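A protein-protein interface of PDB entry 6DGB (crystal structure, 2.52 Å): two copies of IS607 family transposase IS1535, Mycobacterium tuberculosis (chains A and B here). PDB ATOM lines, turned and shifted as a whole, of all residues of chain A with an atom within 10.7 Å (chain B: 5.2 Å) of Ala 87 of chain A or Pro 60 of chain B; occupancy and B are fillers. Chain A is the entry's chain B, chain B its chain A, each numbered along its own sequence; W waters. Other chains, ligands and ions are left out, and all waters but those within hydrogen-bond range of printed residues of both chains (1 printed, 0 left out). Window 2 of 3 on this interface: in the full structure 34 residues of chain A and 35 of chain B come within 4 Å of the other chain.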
ATOM      1  N   PRO A  60     -19.437  34.256 -15.830  1.00  0.00           N
ATOM      2  CA  PRO A  60     -20.398  33.190 -15.461  1.00  0.00           C
ATOM      3  C   PRO A  60     -21.522  32.969 -16.463  1.00  0.00           C
ATOM      4  O   PRO A  60     -22.214  31.952 -16.367  1.00  0.00           O
ATOM      5  CB  PRO A  60     -20.969  33.663 -14.127  1.00  0.00           C
ATOM      6  CG  PRO A  60     -20.074  34.759 -13.677  1.00  0.00           C
ATOM      7  CD  PRO A  60     -19.520  35.389 -14.893  1.00  0.00           C
ATOM      8  N   ARG A  63     -22.062  29.738 -20.206  1.00  0.00           N
ATOM      9  CA  ARG A  63     -22.546  28.465 -19.662  1.00  0.00           C
ATOM     10  C   ARG A  63     -22.023  27.298 -20.459  1.00  0.00           C
ATOM     11  O   ARG A  63     -21.739  26.256 -19.883  1.00  0.00           O
ATOM     12  CB  ARG A  63     -24.095  28.395 -19.581  1.00  0.00           C
ATOM     13  CG  ARG A  63     -24.840  29.703 -19.272  1.00  0.00           C
ATOM     14  CD  ARG A  63     -24.706  30.225 -17.836  1.00  0.00           C
ATOM     15  NE  ARG A  63     -24.978  29.167 -16.865  1.00  0.00           N
ATOM     16  CZ  ARG A  63     -24.619  29.168 -15.586  1.00  0.00           C
ATOM     17  NH1 ARG A  63     -24.880  28.119 -14.820  1.00  0.00           N
ATOM     18  NH2 ARG A  63     -24.001  30.221 -15.059  1.00  0.00           N
ATOM     19  N   GLU A  79      -9.782  18.286 -17.326  1.00  0.00           N
ATOM     20  CA  GLU A  79     -10.644  17.586 -16.377  1.00  0.00           C
ATOM     21  C   GLU A  79     -10.937  18.411 -15.097  1.00  0.00           C
ATOM     22  O   GLU A  79     -12.058  18.350 -14.570  1.00  0.00           O
ATOM     23  CB  GLU A  79     -10.090  16.187 -16.038  1.00  0.00           C
ATOM     24  CG  GLU A  79      -8.634  16.147 -15.576  1.00  0.00           C
ATOM     25  CD  GLU A  79      -8.208  14.866 -14.871  1.00  0.00           C
ATOM     26  OE1 GLU A  79      -8.482  13.770 -15.414  1.00  0.00           O
ATOM     27  OE2 GLU A  79      -7.583  14.957 -13.787  1.00  0.00           O
ATOM     28  N   HIS A  80      -9.936  19.223 -14.646  1.00  0.00           N
ATOM     29  CA  HIS A  80     -10.021  20.093 -13.467  1.00  0.00           C
ATOM     30  C   HIS A  80     -10.831  21.342 -13.733  1.00  0.00           C
ATOM     31  O   HIS A  80     -11.596  21.755 -12.859  1.00  0.00           O
ATOM     32  CB  HIS A  80      -8.627  20.412 -12.899  1.00  0.00           C
ATOM     33  CG  HIS A  80      -7.859  19.181 -12.500  1.00  0.00           C
ATOM     34  ND1 HIS A  80      -8.380  18.265 -11.588  1.00  0.00           N
ATOM     35  CD2 HIS A  80      -6.664  18.727 -12.944  1.00  0.00           C
ATOM     36  CE1 HIS A  80      -7.481  17.301 -11.494  1.00  0.00           C
ATOM     37  NE2 HIS A  80      -6.437  17.525 -12.302  1.00  0.00           N
ATOM     38  N   LEU A  81     -10.686  21.927 -14.948  1.00  0.00           N
ATOM     39  CA  LEU A  81     -11.473  23.071 -15.399  1.00  0.00           C
ATOM     40  C   LEU A  81     -12.951  22.665 -15.433  1.00  0.00           C
ATOM     41  O   LEU A  81     -13.788  23.400 -14.903  1.00  0.00           O
ATOM     42  CB  LEU A  81     -11.055  23.523 -16.815  1.00  0.00           C
ATOM     43  CG  LEU A  81      -9.905  24.499 -16.936  1.00  0.00           C
ATOM     44  CD1 LEU A  81      -9.659  24.836 -18.392  1.00  0.00           C
ATOM     45  CD2 LEU A  81     -10.195  25.778 -16.191  1.00  0.00           C
ATOM     46  N   GLU A  82     -13.256  21.468 -16.024  1.00  0.00           N
ATOM     47  CA  GLU A  82     -14.607  20.892 -16.135  1.00  0.00           C
ATOM     48  C   GLU A  82     -15.207  20.719 -14.764  1.00  0.00           C
ATOM     49  O   GLU A  82     -16.384  21.060 -14.584  1.00  0.00           O
ATOM     50  CB  GLU A  82     -14.613  19.544 -16.889  1.00  0.00           C
ATOM     51  CG  GLU A  82     -14.477  19.659 -18.394  1.00  0.00           C
ATOM     52  CD  GLU A  82     -14.406  18.331 -19.111  1.00  0.00           C
ATOM     53  OE1 GLU A  82     -13.316  17.710 -19.109  1.00  0.00           O
ATOM     54  OE2 GLU A  82     -15.436  17.918 -19.697  1.00  0.00           O
ATOM     55  N   ALA A  83     -14.384  20.229 -13.790  1.00  0.00           N
ATOM     56  CA  ALA A  83     -14.788  20.032 -12.404  1.00  0.00           C
ATOM     57  C   ALA A  83     -15.140  21.364 -11.750  1.00  0.00           C
ATOM     58  O   ALA A  83     -16.213  21.479 -11.175  1.00  0.00           O
ATOM     59  CB  ALA A  83     -13.689  19.335 -11.627  1.00  0.00           C
ATOM     60  N   ALA A  84     -14.272  22.381 -11.868  1.00  0.00           N
ATOM     61  CA  ALA A  84     -14.525  23.708 -11.309  1.00  0.00           C
ATOM     62  C   ALA A  84     -15.813  24.335 -11.913  1.00  0.00           C
ATOM     63  O   ALA A  84     -16.633  24.869 -11.162  1.00  0.00           O
ATOM     64  CB  ALA A  84     -13.319  24.603 -11.563  1.00  0.00           C
ATOM     65  N   LEU A  85     -15.995  24.228 -13.262  1.00  0.00           N
ATOM     66  CA  LEU A  85     -17.140  24.774 -14.008  1.00  0.00           C
ATOM     67  C   LEU A  85     -18.450  24.094 -13.652  1.00  0.00           C
ATOM     68  O   LEU A  85     -19.480  24.766 -13.521  1.00  0.00           O
ATOM     69  CB  LEU A  85     -16.901  24.706 -15.543  1.00  0.00           C
ATOM     70  CG  LEU A  85     -15.867  25.695 -16.081  1.00  0.00           C
ATOM     71  CD1 LEU A  85     -15.498  25.383 -17.493  1.00  0.00           C
ATOM     72  CD2 LEU A  85     -16.337  27.122 -15.954  1.00  0.00           C
ATOM     73  N   SER A  86     -18.398  22.745 -13.516  1.00  0.00           N
ATOM     74  CA  SER A  86     -19.529  21.901 -13.159  1.00  0.00           C
ATOM     75  C   SER A  86     -20.210  22.468 -11.909  1.00  0.00           C
ATOM     76  O   SER A  86     -21.431  22.660 -11.943  1.00  0.00           O
ATOM     77  CB  SER A  86     -19.077  20.461 -12.943  1.00  0.00           C
ATOM     78  OG  SER A  86     -18.493  20.257 -11.668  1.00  0.00           O
ATOM     79  N   ALA A  87     -19.409  22.812 -10.846  1.00  0.00           N
ATOM     80  CA  ALA A  87     -19.881  23.439  -9.592  1.00  0.00           C
ATOM     81  C   ALA A  87     -20.738  24.743  -9.814  1.00  0.00           C
ATOM     82  O   ALA A  87     -21.516  25.120  -8.934  1.00  0.00           O
ATOM     83  CB  ALA A  87     -18.703  23.734  -8.671  1.00  0.00           C
ATOM     84  N   GLN A  88     -20.597  25.399 -10.982  1.00  0.00           N
ATOM     85  CA  GLN A  88     -21.341  26.600 -11.329  1.00  0.00           C
ATOM     86  C   GLN A  88     -22.345  26.344 -12.471  1.00  0.00           C
ATOM     87  O   GLN A  88     -22.882  27.293 -13.044  1.00  0.00           O
ATOM     88  CB  GLN A  88     -20.389  27.759 -11.671  1.00  0.00           C
ATOM     89  CG  GLN A  88     -21.024  29.125 -11.383  1.00  0.00           C
ATOM     90  CD  GLN A  88     -20.282  30.326 -11.904  1.00  0.00           C
ATOM     91  OE1 GLN A  88     -19.302  30.230 -12.653  1.00  0.00           O
ATOM     92  NE2 GLN A  88     -20.759  31.500 -11.511  1.00  0.00           N
ATOM     93  N   GLY A  89     -22.604  25.063 -12.762  1.00  0.00           N
ATOM     94  CA  GLY A  89     -23.536  24.605 -13.791  1.00  0.00           C
ATOM     95  C   GLY A  89     -23.169  24.987 -15.212  1.00  0.00           C
ATOM     96  O   GLY A  89     -24.045  25.106 -16.081  1.00  0.00           O
ATOM     97  N   ARG A  90     -21.863  25.196 -15.438  1.00  0.00           N
ATOM     98  CA  ARG A  90     -21.267  25.559 -16.725  1.00  0.00           C
ATOM     99  C   ARG A  90     -20.490  24.339 -17.237  1.00  0.00           C
ATOM    100  O   ARG A  90     -19.993  23.542 -16.420  1.00  0.00           O
ATOM    101  CB  ARG A  90     -20.333  26.773 -16.569  1.00  0.00           C
ATOM    102  CG  ARG A  90     -20.999  28.028 -16.022  1.00  0.00           C
ATOM    103  CD  ARG A  90     -19.987  29.067 -15.603  1.00  0.00           C
ATOM    104  NE  ARG A  90     -19.222  29.580 -16.745  1.00  0.00           N
ATOM    105  CZ  ARG A  90     -18.012  30.130 -16.664  1.00  0.00           C
ATOM    106  NH1 ARG A  90     -17.412  30.263 -15.491  1.00  0.00           N
ATOM    107  NH2 ARG A  90     -17.392  30.550 -17.760  1.00  0.00           N
ATOM    108  N   ARG A  91     -20.396  24.180 -18.580  1.00  0.00           N
ATOM    109  CA  ARG A  91     -19.704  23.028 -19.155  1.00  0.00           C
ATOM    110  C   ARG A  91     -18.931  23.309 -20.454  1.00  0.00           C
ATOM    111  O   ARG A  91     -19.175  24.290 -21.149  1.00  0.00           O
ATOM    112  CB  ARG A  91     -20.669  21.833 -19.347  1.00  0.00           C
ATOM    113  CG  ARG A  91     -21.746  22.041 -20.382  1.00  0.00           C
ATOM    114  CD  ARG A  91     -22.602  20.807 -20.543  1.00  0.00           C
ATOM    115  NE  ARG A  91     -23.641  21.016 -21.556  1.00  0.00           N
ATOM    116  CZ  ARG A  91     -24.822  21.579 -21.316  1.00  0.00           C
ATOM    117  NH1 ARG A  91     -25.134  21.994 -20.090  1.00  0.00           N
ATOM    118  NH2 ARG A  91     -25.701  21.735 -22.297  1.00  0.00           N
ATOM    119  N   ILE A  92     -17.987  22.403 -20.757  1.00  0.00           N
ATOM    120  CA  ILE A  92     -17.148  22.390 -21.950  1.00  0.00           C
ATOM    121  C   ILE A  92     -17.687  21.325 -22.898  1.00  0.00           C
ATOM    122  O   ILE A  92     -17.818  20.154 -22.516  1.00  0.00           O
ATOM    123  CB  ILE A  92     -15.672  22.126 -21.554  1.00  0.00           C
ATOM    124  CG1 ILE A  92     -15.079  23.362 -20.853  1.00  0.00           C
ATOM    125  CG2 ILE A  92     -14.821  21.712 -22.781  1.00  0.00           C
ATOM    126  CD1 ILE A  92     -14.294  23.073 -19.800  1.00  0.00           C
ATOM    127  N   LEU B  57     -12.741  20.860  -6.295  1.00  0.00           N
ATOM    128  CA  LEU B  57     -13.129  21.834  -7.313  1.00  0.00           C
ATOM    129  C   LEU B  57     -14.613  21.785  -7.655  1.00  0.00           C
ATOM    130  O   LEU B  57     -15.209  22.838  -7.884  1.00  0.00           O
ATOM    131  CB  LEU B  57     -12.265  21.745  -8.575  1.00  0.00           C
ATOM    132  CG  LEU B  57     -10.783  22.076  -8.401  1.00  0.00           C
ATOM    133  CD1 LEU B  57      -9.991  21.738  -9.659  1.00  0.00           C
ATOM    134  CD2 LEU B  57     -10.569  23.486  -7.902  1.00  0.00           C
ATOM    135  N   SER B  58     -15.224  20.591  -7.639  1.00  0.00           N
ATOM    136  CA  SER B  58     -16.653  20.449  -7.928  1.00  0.00           C
ATOM    137  C   SER B  58     -17.544  20.836  -6.739  1.00  0.00           C
ATOM    138  O   SER B  58     -18.737  21.024  -6.936  1.00  0.00           O
ATOM    139  CB  SER B  58     -16.976  19.048  -8.431  1.00  0.00           C
ATOM    140  OG  SER B  58     -16.611  18.048  -7.497  1.00  0.00           O
ATOM    141  N   ASP B  59     -16.972  20.988  -5.516  1.00  0.00           N
ATOM    142  CA  ASP B  59     -17.730  21.403  -4.332  1.00  0.00           C
ATOM    143  C   ASP B  59     -17.772  22.930  -4.253  1.00  0.00           C
ATOM    144  O   ASP B  59     -16.734  23.536  -4.010  1.00  0.00           O
ATOM    145  CB  ASP B  59     -17.163  20.784  -3.035  1.00  0.00           C
ATOM    146  CG  ASP B  59     -17.776  21.330  -1.751  1.00  0.00           C
ATOM    147  OD1 ASP B  59     -19.035  21.353  -1.649  1.00  0.00           O
ATOM    148  OD2 ASP B  59     -17.001  21.728  -0.846  1.00  0.00           O
ATOM    149  N   PRO B  60     -18.950  23.570  -4.449  1.00  0.00           N
ATOM    150  CA  PRO B  60     -19.008  25.050  -4.396  1.00  0.00           C
ATOM    151  C   PRO B  60     -18.767  25.650  -3.014  1.00  0.00           C
ATOM    152  O   PRO B  60     -18.548  26.861  -2.917  1.00  0.00           O
ATOM    153  CB  PRO B  60     -20.423  25.376  -4.878  1.00  0.00           C
ATOM    154  CG  PRO B  60     -20.939  24.106  -5.467  1.00  0.00           C
ATOM    155  CD  PRO B  60     -20.272  22.995  -4.751  1.00  0.00           C
ATOM    156  N   ASP B  61     -18.830  24.814  -1.953  1.00  0.00           N
ATOM    157  CA  ASP B  61     -18.600  25.222  -0.569  1.00  0.00           C
ATOM    158  C   ASP B  61     -17.120  25.490  -0.287  1.00  0.00           C
ATOM    159  O   ASP B  61     -16.829  26.192   0.687  1.00  0.00           O
ATOM    160  CB  ASP B  61     -19.113  24.149   0.410  1.00  0.00           C
ATOM    161  CG  ASP B  61     -20.614  24.082   0.595  1.00  0.00           C
ATOM    162  OD1 ASP B  61     -21.337  24.862  -0.079  1.00  0.00           O
ATOM    163  OD2 ASP B  61     -21.070  23.257   1.421  1.00  0.00           O
ATOM    164  N   ALA B  62     -16.186  24.886  -1.093  1.00  0.00           N
ATOM    165  CA  ALA B  62     -14.729  25.045  -0.959  1.00  0.00           C
ATOM    166  C   ALA B  62     -14.387  26.396  -1.588  1.00  0.00           C
ATOM    167  O   ALA B  62     -13.965  26.468  -2.750  1.00  0.00           O
ATOM    168  CB  ALA B  62     -14.001  23.896  -1.658  1.00  0.00           C
ATOM    169  N   ARG B  63     -14.684  27.482  -0.837  1.00  0.00           N
ATOM    170  CA  ARG B  63     -14.501  28.867  -1.276  1.00  0.00           C
ATOM    171  C   ARG B  63     -13.027  29.236  -1.349  1.00  0.00           C
ATOM    172  O   ARG B  63     -12.645  29.995  -2.227  1.00  0.00           O
ATOM    173  CB  ARG B  63     -15.274  29.844  -0.370  1.00  0.00           C
ATOM    174  CG  ARG B  63     -15.641  31.179  -1.048  1.00  0.00           C
ATOM    175  CD  ARG B  63     -17.115  31.512  -0.937  1.00  0.00           C
ATOM    176  NE  ARG B  63     -17.915  30.473  -1.572  1.00  0.00           N
ATOM    177  CZ  ARG B  63     -18.537  30.596  -2.736  1.00  0.00           C
ATOM    178  NH1 ARG B  63     -18.489  31.742  -3.404  1.00  0.00           N
ATOM    179  NH2 ARG B  63     -19.220  29.577  -3.240  1.00  0.00           N
ATOM    180  N   GLN B  88     -17.299  32.135  -9.638  1.00  0.00           N
ATOM    181  CA  GLN B  88     -18.149  31.594  -8.590  1.00  0.00           C
ATOM    182  C   GLN B  88     -17.755  32.124  -7.194  1.00  0.00           C
ATOM    183  O   GLN B  88     -18.203  31.585  -6.187  1.00  0.00           O
ATOM    184  CB  GLN B  88     -18.156  30.058  -8.636  1.00  0.00           C
ATOM    185  CG  GLN B  88     -19.463  29.482  -8.093  1.00  0.00           C
ATOM    186  CD  GLN B  88     -19.491  27.993  -7.849  1.00  0.00           C
ATOM    187  OE1 GLN B  88     -18.479  27.285  -7.942  1.00  0.00           O
ATOM    188  NE2 GLN B  88     -20.678  27.488  -7.526  1.00  0.00           N
ATOM    189  N   ARG B  90     -14.934  31.978  -5.645  1.00  0.00           N
ATOM    190  CA  ARG B  90     -14.032  31.033  -4.992  1.00  0.00           C
ATOM    191  C   ARG B  90     -12.602  31.362  -5.444  1.00  0.00           C
ATOM    192  O   ARG B  90     -12.408  31.876  -6.564  1.00  0.00           O
ATOM    193  CB  ARG B  90     -14.406  29.584  -5.372  1.00  0.00           C
ATOM    194  CG  ARG B  90     -15.836  29.171  -5.004  1.00  0.00           C
ATOM    195  CD  ARG B  90     -16.236  27.879  -5.674  1.00  0.00           C
ATOM    196  NE  ARG B  90     -15.445  26.754  -5.186  1.00  0.00           N
ATOM    197  CZ  ARG B  90     -15.252  25.624  -5.858  1.00  0.00           C
ATOM    198  NH1 ARG B  90     -15.809  25.449  -7.057  1.00  0.00           N
ATOM    199  NH2 ARG B  90     -14.502  24.656  -5.340  1.00  0.00           N
HETATM  200  O   HOH W   1     -16.970  27.451 -10.210  1.00  0.00           O
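Printed residues of chain A that touch a printed residue of chain B: His 80, Ala 83, Ala 84, Ser 86, Ala 87 and Gln 88. Hydrophobic or aromatic side chains of chain B that line the printed part of chain A: Leu 57 and Pro 60. Among the printed residues, 11 pairs touch across the chains.
The backbone carbonyl oxygen of Ala 87 of chain A is in hydrogen-bond range of the side-chain amide nitrogen of Gln 88 of chain B (2.9 Å).
Gln 88 of chain A touches its own counterpart, Gln 88 of chain B. Positions printed for both chains: 60, 63, 88 and 90.
Of chain B, only Leu 57 (3.7 Å), Ser 58 (3.2 Å), Pro 60 (3.7 Å), Gln 88 (2.9 Å) and Arg 90 (3.7 Å) come within 4 Å of Ala 87 of chain A. Pro 60 of chain B touches just one residue of chain A: Ala 87. Ser 58 of chain B touches three residues of chain A. No residue of chain A comes within 4 Å of Asp 59 of chain B. No residue of chain A comes within 4 Å of Asp 61 of chain B. Ala 62 of chain B touches none of the printed residues of chain A. Of the printed residues of chain B, Ala 84 of chain A touches Leu 57. Printed residues of chain B within 4 Å of Ser 86 of chain A: Ser 58. Printed residues of chain A within 4 Å of Gln 88 of chain B: Ala 87 (2.9 Å) and Gln 88 (3.7 Å). Of the printed residues of chain B, His 80 of chain A touches Leu 57 (3.6 Å). Printed residues of chain B within 4 Å of Gln 88 of chain A: Gln 88 (3.7 Å). The nearest residue of chain B that does not touch Ala 87 of chain A is Asp 59 of chain B (4.5 Å). The nearest residue of chain A that does not touch Pro 60 of chain B is Gln 88 of chain A (5.7 Å).
Water W1 lies within hydrogen-bond range of OE1 of Gln 88 of chain B (2.7 Å) and O of Ala 84 of chain A (2.8 Å).
NH1 of Arg 90 of chain B is in hydrogen-bond range of O of Leu 57 of chain B (2.8 Å). The backbone carbonyl oxygen of Ala 62 of chain B sits at hydrogen-bond distance from the guanidinium group of Arg 90 of chain B (2.9 Å). The guanidinium group of Arg 63 of chain B sits at hydrogen-bond distance from the backbone carbonyl oxygen of Gln 88 of chain B (2.8 Å). NH1 of Arg 90 of chain B lies close to OE1 of Gln 88 of chain B (3.4 Å). NE2 of His 80 of chain A lies within hydrogen-bond range of OE2 of Glu 79 of chain A (3.2 Å). OG of Ser 86 of chain A sits at hydrogen-bond distance from O of Ala 83 of chain A.
Among the printed residues, pairs that only touch across the chains: Ala 87 of chain A with Ser 58 of chain B, Ala 83 of chain A with Ser 58 of chain B, His 80 of chain A with Leu 57 of chain B, Ala 84 of chain A with Leu 57 of chain B, Ala 87 of chain A with Pro 60 of chain B, Gln 88 of chain A with Gln 88 of chain B, Ala 87 of chain A with Leu 57 of chain B, Ala 83 of chain A with Leu 57 of chain B, Ala 87 of chain A with Arg 90 of chain B and Ser 86 of chain A with Ser 58 of chain B.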
